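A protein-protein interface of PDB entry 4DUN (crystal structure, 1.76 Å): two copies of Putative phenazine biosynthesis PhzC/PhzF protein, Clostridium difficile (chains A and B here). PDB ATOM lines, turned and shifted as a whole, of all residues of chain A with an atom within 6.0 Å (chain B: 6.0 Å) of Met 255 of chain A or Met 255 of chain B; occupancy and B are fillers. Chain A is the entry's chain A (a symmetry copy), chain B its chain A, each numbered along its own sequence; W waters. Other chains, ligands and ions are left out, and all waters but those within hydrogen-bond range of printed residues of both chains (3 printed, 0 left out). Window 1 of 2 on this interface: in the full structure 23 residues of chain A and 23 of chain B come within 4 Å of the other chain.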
ATOM      1  N   TYR A   6       5.702  24.525  28.250  1.00  0.00           N
ATOM      2  CA  TYR A   6       5.193  23.449  27.400  1.00  0.00           C
ATOM      3  C   TYR A   6       6.242  22.351  27.275  1.00  0.00           C
ATOM      4  O   TYR A   6       7.442  22.633  27.145  1.00  0.00           O
ATOM      5  CB  TYR A   6       4.769  24.003  26.015  1.00  0.00           C
ATOM      6  CG  TYR A   6       4.261  22.917  25.092  1.00  0.00           C
ATOM      7  CD1 TYR A   6       3.093  22.217  25.384  1.00  0.00           C
ATOM      8  CD2 TYR A   6       5.009  22.504  23.991  1.00  0.00           C
ATOM      9  CE1 TYR A   6       2.674  21.143  24.598  1.00  0.00           C
ATOM     10  CE2 TYR A   6       4.595  21.438  23.194  1.00  0.00           C
ATOM     11  CZ  TYR A   6       3.430  20.756  23.507  1.00  0.00           C
ATOM     12  OH  TYR A   6       3.004  19.717  22.723  1.00  0.00           O
ATOM     13  N   TYR A   7       5.779  21.097  27.369  1.00  0.00           N
ATOM     14  CA  TYR A   7       6.609  19.906  27.385  1.00  0.00           C
ATOM     15  C   TYR A   7       6.029  18.833  26.504  1.00  0.00           C
ATOM     16  O   TYR A   7       4.807  18.653  26.481  1.00  0.00           O
ATOM     17  CB  TYR A   7       6.685  19.331  28.834  1.00  0.00           C
ATOM     18  CG  TYR A   7       7.120  20.322  29.888  1.00  0.00           C
ATOM     19  CD1 TYR A   7       6.200  21.174  30.498  1.00  0.00           C
ATOM     20  CD2 TYR A   7       8.447  20.390  30.305  1.00  0.00           C
ATOM     21  CE1 TYR A   7       6.601  22.109  31.458  1.00  0.00           C
ATOM     22  CE2 TYR A   7       8.854  21.304  31.277  1.00  0.00           C
ATOM     23  CZ  TYR A   7       7.928  22.157  31.853  1.00  0.00           C
ATOM     24  OH  TYR A   7       8.340  23.054  32.813  1.00  0.00           O
ATOM     25  N   ILE A   8       6.894  18.083  25.822  1.00  0.00           N
ATOM     26  CA  ILE A   8       6.501  16.888  25.071  1.00  0.00           C
ATOM     27  C   ILE A   8       7.125  15.723  25.815  1.00  0.00           C
ATOM     28  O   ILE A   8       8.344  15.686  25.973  1.00  0.00           O
ATOM     29  CB  ILE A   8       6.882  16.881  23.573  1.00  0.00           C
ATOM     30  CG1 ILE A   8       6.224  18.056  22.821  1.00  0.00           C
ATOM     31  CG2 ILE A   8       6.486  15.511  22.961  1.00  0.00           C
ATOM     32  CD1 ILE A   8       6.770  18.268  21.377  1.00  0.00           C
ATOM     33  N   VAL A   9       6.290  14.805  26.302  1.00  0.00           N
ATOM     34  CA  VAL A   9       6.719  13.689  27.149  1.00  0.00           C
ATOM     35  C   VAL A   9       6.214  12.377  26.588  1.00  0.00           C
ATOM     36  O   VAL A   9       5.038  12.287  26.217  1.00  0.00           O
ATOM     37  CB  VAL A   9       6.158  13.914  28.599  1.00  0.00           C
ATOM     38  CG1 VAL A   9       6.431  12.721  29.530  1.00  0.00           C
ATOM     39  CG2 VAL A   9       6.682  15.216  29.210  1.00  0.00           C
ATOM     40  N   ASN A  43      -0.379  21.547  18.203  1.00  0.00           N
ATOM     41  CA  ASN A  43       0.590  20.525  18.582  1.00  0.00           C
ATOM     42  C   ASN A  43       0.459  19.259  17.718  1.00  0.00           C
ATOM     43  O   ASN A  43       1.474  18.644  17.360  1.00  0.00           O
ATOM     44  CB  ASN A  43       0.419  20.166  20.049  1.00  0.00           C
ATOM     45  CG  ASN A  43       0.933  21.243  20.959  1.00  0.00           C
ATOM     46  OD1 ASN A  43       1.867  21.972  20.627  1.00  0.00           O
ATOM     47  ND2 ASN A  43       0.368  21.324  22.162  1.00  0.00           N
ATOM     48  N   LEU A 253      11.411  12.901  28.792  1.00  0.00           N
ATOM     49  CA  LEU A 253      11.206  14.252  28.235  1.00  0.00           C
ATOM     50  C   LEU A 253      11.806  14.325  26.843  1.00  0.00           C
ATOM     51  O   LEU A 253      12.989  14.037  26.670  1.00  0.00           O
ATOM     52  CB  LEU A 253      11.848  15.326  29.144  1.00  0.00           C
ATOM     53  CG  LEU A 253      11.735  16.784  28.665  1.00  0.00           C
ATOM     54  CD1 LEU A 253      10.291  17.253  28.670  1.00  0.00           C
ATOM     55  CD2 LEU A 253      12.611  17.698  29.488  1.00  0.00           C
ATOM     56  N   PHE A 254      11.007  14.757  25.853  1.00  0.00           N
ATOM     57  CA  PHE A 254      11.508  14.957  24.493  1.00  0.00           C
ATOM     58  C   PHE A 254      11.884  16.424  24.262  1.00  0.00           C
ATOM     59  O   PHE A 254      12.927  16.711  23.685  1.00  0.00           O
ATOM     60  CB  PHE A 254      10.458  14.510  23.436  1.00  0.00           C
ATOM     61  CG  PHE A 254      10.769  14.987  22.027  1.00  0.00           C
ATOM     62  CD1 PHE A 254      11.908  14.542  21.357  1.00  0.00           C
ATOM     63  CD2 PHE A 254       9.907  15.861  21.366  1.00  0.00           C
ATOM     64  CE1 PHE A 254      12.179  14.962  20.045  1.00  0.00           C
ATOM     65  CE2 PHE A 254      10.177  16.279  20.051  1.00  0.00           C
ATOM     66  CZ  PHE A 254      11.313  15.832  19.405  1.00  0.00           C
ATOM     67  N   MET A 255      11.021  17.351  24.685  1.00  0.00           N
ATOM     68  CA  MET A 255      11.201  18.757  24.363  1.00  0.00           C
ATOM     69  C   MET A 255      10.616  19.607  25.485  1.00  0.00           C
ATOM     70  O   MET A 255       9.555  19.273  26.019  1.00  0.00           O
ATOM     71  CB  MET A 255      10.470  19.027  23.009  1.00  0.00           C
ATOM     72  CG  MET A 255      10.810  20.359  22.324  1.00  0.00           C
ATOM     73  SD  MET A 255      10.020  21.819  23.076  1.00  0.00           S
ATOM     74  CE  MET A 255       8.274  21.312  23.045  1.00  0.00           C
ATOM     75  N   GLN A 256      11.317  20.672  25.857  1.00  0.00           N
ATOM     76  CA  GLN A 256      10.873  21.639  26.865  1.00  0.00           C
ATOM     77  C   GLN A 256      10.919  23.033  26.233  1.00  0.00           C
ATOM     78  O   GLN A 256      11.934  23.415  25.668  1.00  0.00           O
ATOM     79  CB  GLN A 256      11.740  21.557  28.130  1.00  0.00           C
ATOM     80  CG  GLN A 256      11.545  22.704  29.123  1.00  0.00           C
ATOM     81  CD  GLN A 256      12.416  22.587  30.356  1.00  0.00           C
ATOM     82  OE1 GLN A 256      13.435  21.879  30.388  1.00  0.00           O
ATOM     83  NE2 GLN A 256      12.019  23.277  31.408  1.00  0.00           N
ATOM     84  N   GLY A 257       9.816  23.765  26.315  1.00  0.00           N
ATOM     85  CA  GLY A 257       9.743  25.098  25.739  1.00  0.00           C
ATOM     86  C   GLY A 257       8.653  25.975  26.300  1.00  0.00           C
ATOM     87  O   GLY A 257       8.145  25.732  27.397  1.00  0.00           O
ATOM     88  N   THR A 258       8.314  27.020  25.551  1.00  0.00           N
ATOM     89  CA  THR A 258       7.265  27.961  25.956  1.00  0.00           C
ATOM     90  C   THR A 258       6.354  28.265  24.782  1.00  0.00           C
ATOM     91  O   THR A 258       6.830  28.428  23.660  1.00  0.00           O
ATOM     92  CB  THR A 258       7.852  29.266  26.521  1.00  0.00           C
ATOM     93  OG1 THR A 258       8.656  29.885  25.522  1.00  0.00           O
ATOM     94  CG2 THR A 258       8.674  29.058  27.790  1.00  0.00           C
ATOM     95  N   ILE A 259       5.058  28.374  25.044  1.00  0.00           N
ATOM     96  CA  ILE A 259       4.081  28.791  24.035  1.00  0.00           C
ATOM     97  C   ILE A 259       3.914  30.285  24.228  1.00  0.00           C
ATOM     98  O   ILE A 259       3.620  30.741  25.340  1.00  0.00           O
ATOM     99  CB  ILE A 259       2.769  27.979  24.090  1.00  0.00           C
ATOM    100  CG1 ILE A 259       3.032  26.507  23.632  1.00  0.00           C
ATOM    101  CG2 ILE A 259       1.659  28.659  23.277  1.00  0.00           C
ATOM    102  CD1 ILE A 259       1.939  25.524  23.975  1.00  0.00           C
ATOM    103  N   LYS A 260       4.064  31.025  23.125  1.00  0.00           N
ATOM    104  CA  LYS A 260       4.041  32.478  23.049  1.00  0.00           C
ATOM    105  C   LYS A 260       2.614  32.990  22.809  1.00  0.00           C
ATOM    106  O   LYS A 260       2.250  33.315  21.678  1.00  0.00           O
ATOM    107  CB  LYS A 260       5.012  32.960  21.934  1.00  0.00           C
ATOM    108  CG  LYS A 260       6.159  31.979  21.574  1.00  0.00           C
ATOM    109  CD  LYS A 260       7.267  31.837  22.635  1.00  0.00           C
ATOM    110  CE  LYS A 260       8.298  32.937  22.587  1.00  0.00           C
ATOM    111  NZ  LYS A 260       9.516  32.576  23.355  1.00  0.00           N
ATOM    112  N   TYR B   6      14.565  24.391  18.987  1.00  0.00           N
ATOM    113  CA  TYR B   6      13.401  23.885  18.260  1.00  0.00           C
ATOM    114  C   TYR B   6      12.274  24.910  18.311  1.00  0.00           C
ATOM    115  O   TYR B   6      12.040  25.541  19.352  1.00  0.00           O
ATOM    116  CB  TYR B   6      12.958  22.510  18.827  1.00  0.00           C
ATOM    117  CG  TYR B   6      11.738  21.962  18.120  1.00  0.00           C
ATOM    118  CD1 TYR B   6      11.789  21.607  16.775  1.00  0.00           C
ATOM    119  CD2 TYR B   6      10.501  21.912  18.760  1.00  0.00           C
ATOM    120  CE1 TYR B   6      10.645  21.201  16.087  1.00  0.00           C
ATOM    121  CE2 TYR B   6       9.354  21.501  18.085  1.00  0.00           C
ATOM    122  CZ  TYR B   6       9.430  21.154  16.745  1.00  0.00           C
ATOM    123  OH  TYR B   6       8.313  20.734  16.073  1.00  0.00           O
ATOM    124  N   TYR B   7      11.616  25.103  17.160  1.00  0.00           N
ATOM    125  CA  TYR B   7      10.584  26.103  16.953  1.00  0.00           C
ATOM    126  C   TYR B   7       9.422  25.527  16.192  1.00  0.00           C
ATOM    127  O   TYR B   7       9.628  24.746  15.257  1.00  0.00           O
ATOM    128  CB  TYR B   7      11.154  27.289  16.113  1.00  0.00           C
ATOM    129  CG  TYR B   7      12.419  27.906  16.662  1.00  0.00           C
ATOM    130  CD1 TYR B   7      13.670  27.367  16.365  1.00  0.00           C
ATOM    131  CD2 TYR B   7      12.374  29.050  17.455  1.00  0.00           C
ATOM    132  CE1 TYR B   7      14.843  27.920  16.888  1.00  0.00           C
ATOM    133  CE2 TYR B   7      13.539  29.623  17.964  1.00  0.00           C
ATOM    134  CZ  TYR B   7      14.770  29.058  17.676  1.00  0.00           C
ATOM    135  OH  TYR B   7      15.912  29.633  18.183  1.00  0.00           O
ATOM    136  N   ILE B   8       8.207  25.945  16.543  1.00  0.00           N
ATOM    137  CA  ILE B   8       6.997  25.625  15.783  1.00  0.00           C
ATOM    138  C   ILE B   8       6.533  26.942  15.190  1.00  0.00           C
ATOM    139  O   ILE B   8       6.272  27.885  15.934  1.00  0.00           O
ATOM    140  CB  ILE B   8       5.870  24.926  16.577  1.00  0.00           C
ATOM    141  CG1 ILE B   8       6.344  23.577  17.155  1.00  0.00           C
ATOM    142  CG2 ILE B   8       4.636  24.754  15.651  1.00  0.00           C
ATOM    143  CD1 ILE B   8       5.356  22.948  18.182  1.00  0.00           C
ATOM    144  N   VAL B   9       6.475  27.015  13.860  1.00  0.00           N
ATOM    145  CA  VAL B   9       6.170  28.248  13.129  1.00  0.00           C
ATOM    146  C   VAL B   9       5.040  28.014  12.149  1.00  0.00           C
ATOM    147  O   VAL B   9       5.059  27.010  11.429  1.00  0.00           O
ATOM    148  CB  VAL B   9       7.462  28.715  12.370  1.00  0.00           C
ATOM    149  CG1 VAL B   9       7.205  29.923  11.454  1.00  0.00           C
ATOM    150  CG2 VAL B   9       8.614  28.997  13.339  1.00  0.00           C
ATOM    151  N   ASN B  43       7.447  14.884  16.587  1.00  0.00           N
ATOM    152  CA  ASN B  43       6.736  16.150  16.451  1.00  0.00           C
ATOM    153  C   ASN B  43       5.328  15.960  15.864  1.00  0.00           C
ATOM    154  O   ASN B  43       4.381  16.641  16.287  1.00  0.00           O
ATOM    155  CB  ASN B  43       7.534  17.103  15.576  1.00  0.00           C
ATOM    156  CG  ASN B  43       8.738  17.649  16.286  1.00  0.00           C
ATOM    157  OD1 ASN B  43       8.746  17.812  17.506  1.00  0.00           O
ATOM    158  ND2 ASN B  43       9.767  18.008  15.520  1.00  0.00           N
ATOM    159  N   LEU B 253       5.426  32.770  15.210  1.00  0.00           N
ATOM    160  CA  LEU B 253       6.024  31.790  16.138  1.00  0.00           C
ATOM    161  C   LEU B 253       4.961  31.281  17.094  1.00  0.00           C
ATOM    162  O   LEU B 253       4.315  32.077  17.773  1.00  0.00           O
ATOM    163  CB  LEU B 253       7.188  32.426  16.932  1.00  0.00           C
ATOM    164  CG  LEU B 253       7.887  31.521  17.964  1.00  0.00           C
ATOM    165  CD1 LEU B 253       8.615  30.376  17.284  1.00  0.00           C
ATOM    166  CD2 LEU B 253       8.819  32.318  18.845  1.00  0.00           C
ATOM    167  N   PHE B 254       4.810  29.949  17.187  1.00  0.00           N
ATOM    168  CA  PHE B 254       3.884  29.346  18.145  1.00  0.00           C
ATOM    169  C   PHE B 254       4.618  28.930  19.423  1.00  0.00           C
ATOM    170  O   PHE B 254       4.128  29.166  20.522  1.00  0.00           O
ATOM    171  CB  PHE B 254       3.159  28.115  17.530  1.00  0.00           C
ATOM    172  CG  PHE B 254       2.441  27.254  18.554  1.00  0.00           C
ATOM    173  CD1 PHE B 254       1.364  27.758  19.284  1.00  0.00           C
ATOM    174  CD2 PHE B 254       2.830  25.932  18.770  1.00  0.00           C
ATOM    175  CE1 PHE B 254       0.684  26.951  20.209  1.00  0.00           C
ATOM    176  CE2 PHE B 254       2.146  25.123  19.695  1.00  0.00           C
ATOM    177  CZ  PHE B 254       1.085  25.642  20.412  1.00  0.00           C
ATOM    178  N   MET B 255       5.778  28.283  19.281  1.00  0.00           N
ATOM    179  CA  MET B 255       6.463  27.697  20.419  1.00  0.00           C
ATOM    180  C   MET B 255       7.966  27.715  20.162  1.00  0.00           C
ATOM    181  O   MET B 255       8.400  27.455  19.037  1.00  0.00           O
ATOM    182  CB  MET B 255       5.936  26.235  20.586  1.00  0.00           C
ATOM    183  CG  MET B 255       6.281  25.553  21.917  1.00  0.00           C
ATOM    184  SD  MET B 255       8.005  24.977  22.046  1.00  0.00           S
ATOM    185  CE  MET B 255       8.131  23.951  20.550  1.00  0.00           C
ATOM    186  N   GLN B 256       8.744  28.049  21.186  1.00  0.00           N
ATOM    187  CA  GLN B 256      10.210  28.047  21.141  1.00  0.00           C
ATOM    188  C   GLN B 256      10.716  27.175  22.293  1.00  0.00           C
ATOM    189  O   GLN B 256      10.306  27.367  23.430  1.00  0.00           O
ATOM    190  CB  GLN B 256      10.766  29.476  21.219  1.00  0.00           C
ATOM    191  CG  GLN B 256      12.274  29.571  21.463  1.00  0.00           C
ATOM    192  CD  GLN B 256      12.784  30.996  21.532  1.00  0.00           C
ATOM    193  OE1 GLN B 256      12.038  31.960  21.758  1.00  0.00           O
ATOM    194  NE2 GLN B 256      14.078  31.153  21.326  1.00  0.00           N
ATOM    195  N   GLY B 257      11.579  26.218  21.986  1.00  0.00           N
ATOM    196  CA  GLY B 257      12.115  25.323  22.998  1.00  0.00           C
ATOM    197  C   GLY B 257      13.398  24.628  22.619  1.00  0.00           C
ATOM    198  O   GLY B 257      14.119  25.074  21.723  1.00  0.00           O
ATOM    199  N   THR B 258      13.696  23.546  23.329  1.00  0.00           N
ATOM    200  CA  THR B 258      14.905  22.755  23.075  1.00  0.00           C
ATOM    201  C   THR B 258      14.574  21.275  23.077  1.00  0.00           C
ATOM    202  O   THR B 258      13.790  20.821  23.909  1.00  0.00           O
ATOM    203  CB  THR B 258      16.010  23.050  24.106  1.00  0.00           C
ATOM    204  OG1 THR B 258      15.528  22.735  25.408  1.00  0.00           O
ATOM    205  CG2 THR B 258      16.497  24.495  24.071  1.00  0.00           C
ATOM    206  N   ILE B 259      15.190  20.523  22.174  1.00  0.00           N
ATOM    207  CA  ILE B 259      15.064  19.065  22.144  1.00  0.00           C
ATOM    208  C   ILE B 259      16.257  18.541  22.918  1.00  0.00           C
ATOM    209  O   ILE B 259      17.404  18.891  22.610  1.00  0.00           O
ATOM    210  CB  ILE B 259      14.919  18.498  20.715  1.00  0.00           C
ATOM    211  CG1 ILE B 259      13.535  18.910  20.115  1.00  0.00           C
ATOM    212  CG2 ILE B 259      15.143  16.980  20.692  1.00  0.00           C
ATOM    213  CD1 ILE B 259      13.407  18.737  18.621  1.00  0.00           C
ATOM    214  N   LYS B 260      15.971  17.672  23.893  1.00  0.00           N
ATOM    215  CA  LYS B 260      16.913  17.087  24.836  1.00  0.00           C
ATOM    216  C   LYS B 260      17.500  15.781  24.284  1.00  0.00           C
ATOM    217  O   LYS B 260      17.057  14.693  24.654  1.00  0.00           O
ATOM    218  CB  LYS B 260      16.212  16.861  26.205  1.00  0.00           C
ATOM    219  CG  LYS B 260      14.978  17.760  26.484  1.00  0.00           C
ATOM    220  CD  LYS B 260      15.288  19.244  26.760  1.00  0.00           C
ATOM    221  CE  LYS B 260      15.714  19.521  28.181  1.00  0.00           C
ATOM    222  NZ  LYS B 260      15.646  20.970  28.497  1.00  0.00           N
HETATM  223  O   HOH W   1      14.128  24.937  26.478  1.00  0.00           O
HETATM  224  O   HOH W   2      11.271  28.834  25.599  1.00  0.00           O
HETATM  225  O   HOH W   3       4.038  18.693  17.867  1.00  0.00           O
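The backbone NH (N) of Lys 260 of chain A sits at hydrogen-bond distance from the backbone carbonyl oxygen (O) of Phe 254 of chain B (3.2 Å). The backbone carbonyl oxygen (O) of Gln 256 of chain B is in hydrogen-bond range of the backbone NH (N) of Thr 258 of chain A (2.9 Å). OE1 of Gln 256 of chain B lies within hydrogen-bond range of NZ of Lys 260 of chain A. The backbone NH (N) of Thr 258 of chain B sits at hydrogen-bond distance from the backbone carbonyl oxygen (O) of Gln 256 of chain A. The backbone carbonyl oxygen of Phe 254 of chain A is in hydrogen-bond range of the backbone NH of Lys 260 of chain B (3.2 Å). The side-chain amino group (NZ) of Lys 260 of chain B is in hydrogen-bond range of the side-chain amide oxygen (OE1) of Gln 256 of chain A (3.0 Å).
OH of Tyr 6 of chain B lies close to ND2 of Asn 43 of chain B, 3.1 Å away. N of Phe 254 of chain B lies within hydrogen-bond range of O of Ile 8 of chain B (2.8 Å). The side-chain amide nitrogen (ND2) of Asn 43 of chain A sits close to the side-chain hydroxyl (OH) of Tyr 6 of chain A, at 3.1 Å. The backbone NH of Gly 257 of chain A lies within hydrogen-bond range of the backbone carbonyl oxygen of Tyr 6 of chain A. N of Ile 8 of chain A lies within hydrogen-bond range of O of Met 255 of chain A, at 2.9 Å. N of Gly 257 of chain A is in hydrogen-bond range of SD of Met 255 of chain A (3.8 Å).
Among the printed residues, merely in contact across the chains: Tyr 6 of chain A with Met 255 of chain B, Asn 43 of chain A with Asn 43 of chain B, Asn 43 of chain A with Phe 254 of chain B, Leu 253 of chain A with Lys 260 of chain B, Phe 254 of chain A with Asn 43 of chain B, Phe 254 of chain A with Ile 259 of chain B, Met 255 of chain A with Tyr 6 of chain B, Met 255 of chain A with Met 255 of chain B, Met 255 of chain A with Thr 258 of chain B, Met 255 of chain A with Ile 259 of chain B, Gln 256 of chain A with Gly 257 of chain B, Gly 257 of chain A with Gln 256 of chain B, Gly 257 of chain A with Gly 257 of chain B, Thr 258 of chain A with Met 255 of chain B, Ile 259 of chain A with Phe 254 of chain B, Ile 259 of chain A with Met 255 of chain B and Lys 260 of chain A with Leu 253 of chain B.
Of chain A, only Tyr 6 (3.9 Å), Met 255 (3.6 Å), Thr 258 (3.3 Å) and Ile 259 (3.8 Å) come within 4 Å of Met 255 of chain B. Of the printed residues of chain A, Leu 253 of chain B touches Lys 260. Printed residues of chain B within 4 Å of Thr 258 of chain A: Met 255 (3.3 Å) and Gln 256 (2.9 Å). Of the printed residues of chain A, Gln 256 of chain B touches Gly 257, Thr 258 and Lys 260. Ile 8 of chain B touches none of the printed residues of chain A. Tyr 7 of chain A touches none of the printed residues of chain B. The nearest residue of chain A that does not touch Met 255 of chain B is Gly 257 of chain A (4.1 Å). The nearest printed residue of chain A that does not touch Gln 256 of chain B is Gln 256 of chain A (4.8 Å).
Along chain A the printed residues that touch a printed residue of chain B span positions 6 to 260. Of the 13 printed residues of chain B, 10 touch a printed residue of chain A. Along chain B the printed residues that touch a printed residue of chain A span positions 6 to 260. Among the printed residues, 23 pairs touch across the chains.
Asn 43 of chain A touches its own counterpart, Asn 43 of chain B. Met 255 of chain A touches Ile 259 of chain B, and with the chains exchanged Ile 259 of chain A touches Met 255 of chain B. Gln 256 of chain A touches Gly 257 of chain B, and with the chains exchanged Gly 257 of chain A touches Gln 256 of chain B. Gly 257 of chain A touches its own counterpart, Gly 257 of chain B. Positions printed for both chains: 6, 7, 8, 9, 43, 253, 254, 255, 256, 257, 258, 259 and 260. Of the 23 pairs that touch across the chains among the printed residues, 23 have their exchanged pair printed and touching as well.
Water W3 lies within hydrogen-bond range of O of Asn 43 of chain B (2.6 Å) and O of Asn 43 of chain A (2.6 Å). Water W1 lies within hydrogen-bond range of the backbone carbonyl oxygen (O) of Gln 256 of chain A and the side-chain hydroxyl (OG1) of Thr 258 of chain B. Water W2 lies within hydrogen-bond range of O of Gln 256 of chain B (2.8 Å) and OG1 of Thr 258 of chain A (2.8 Å).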
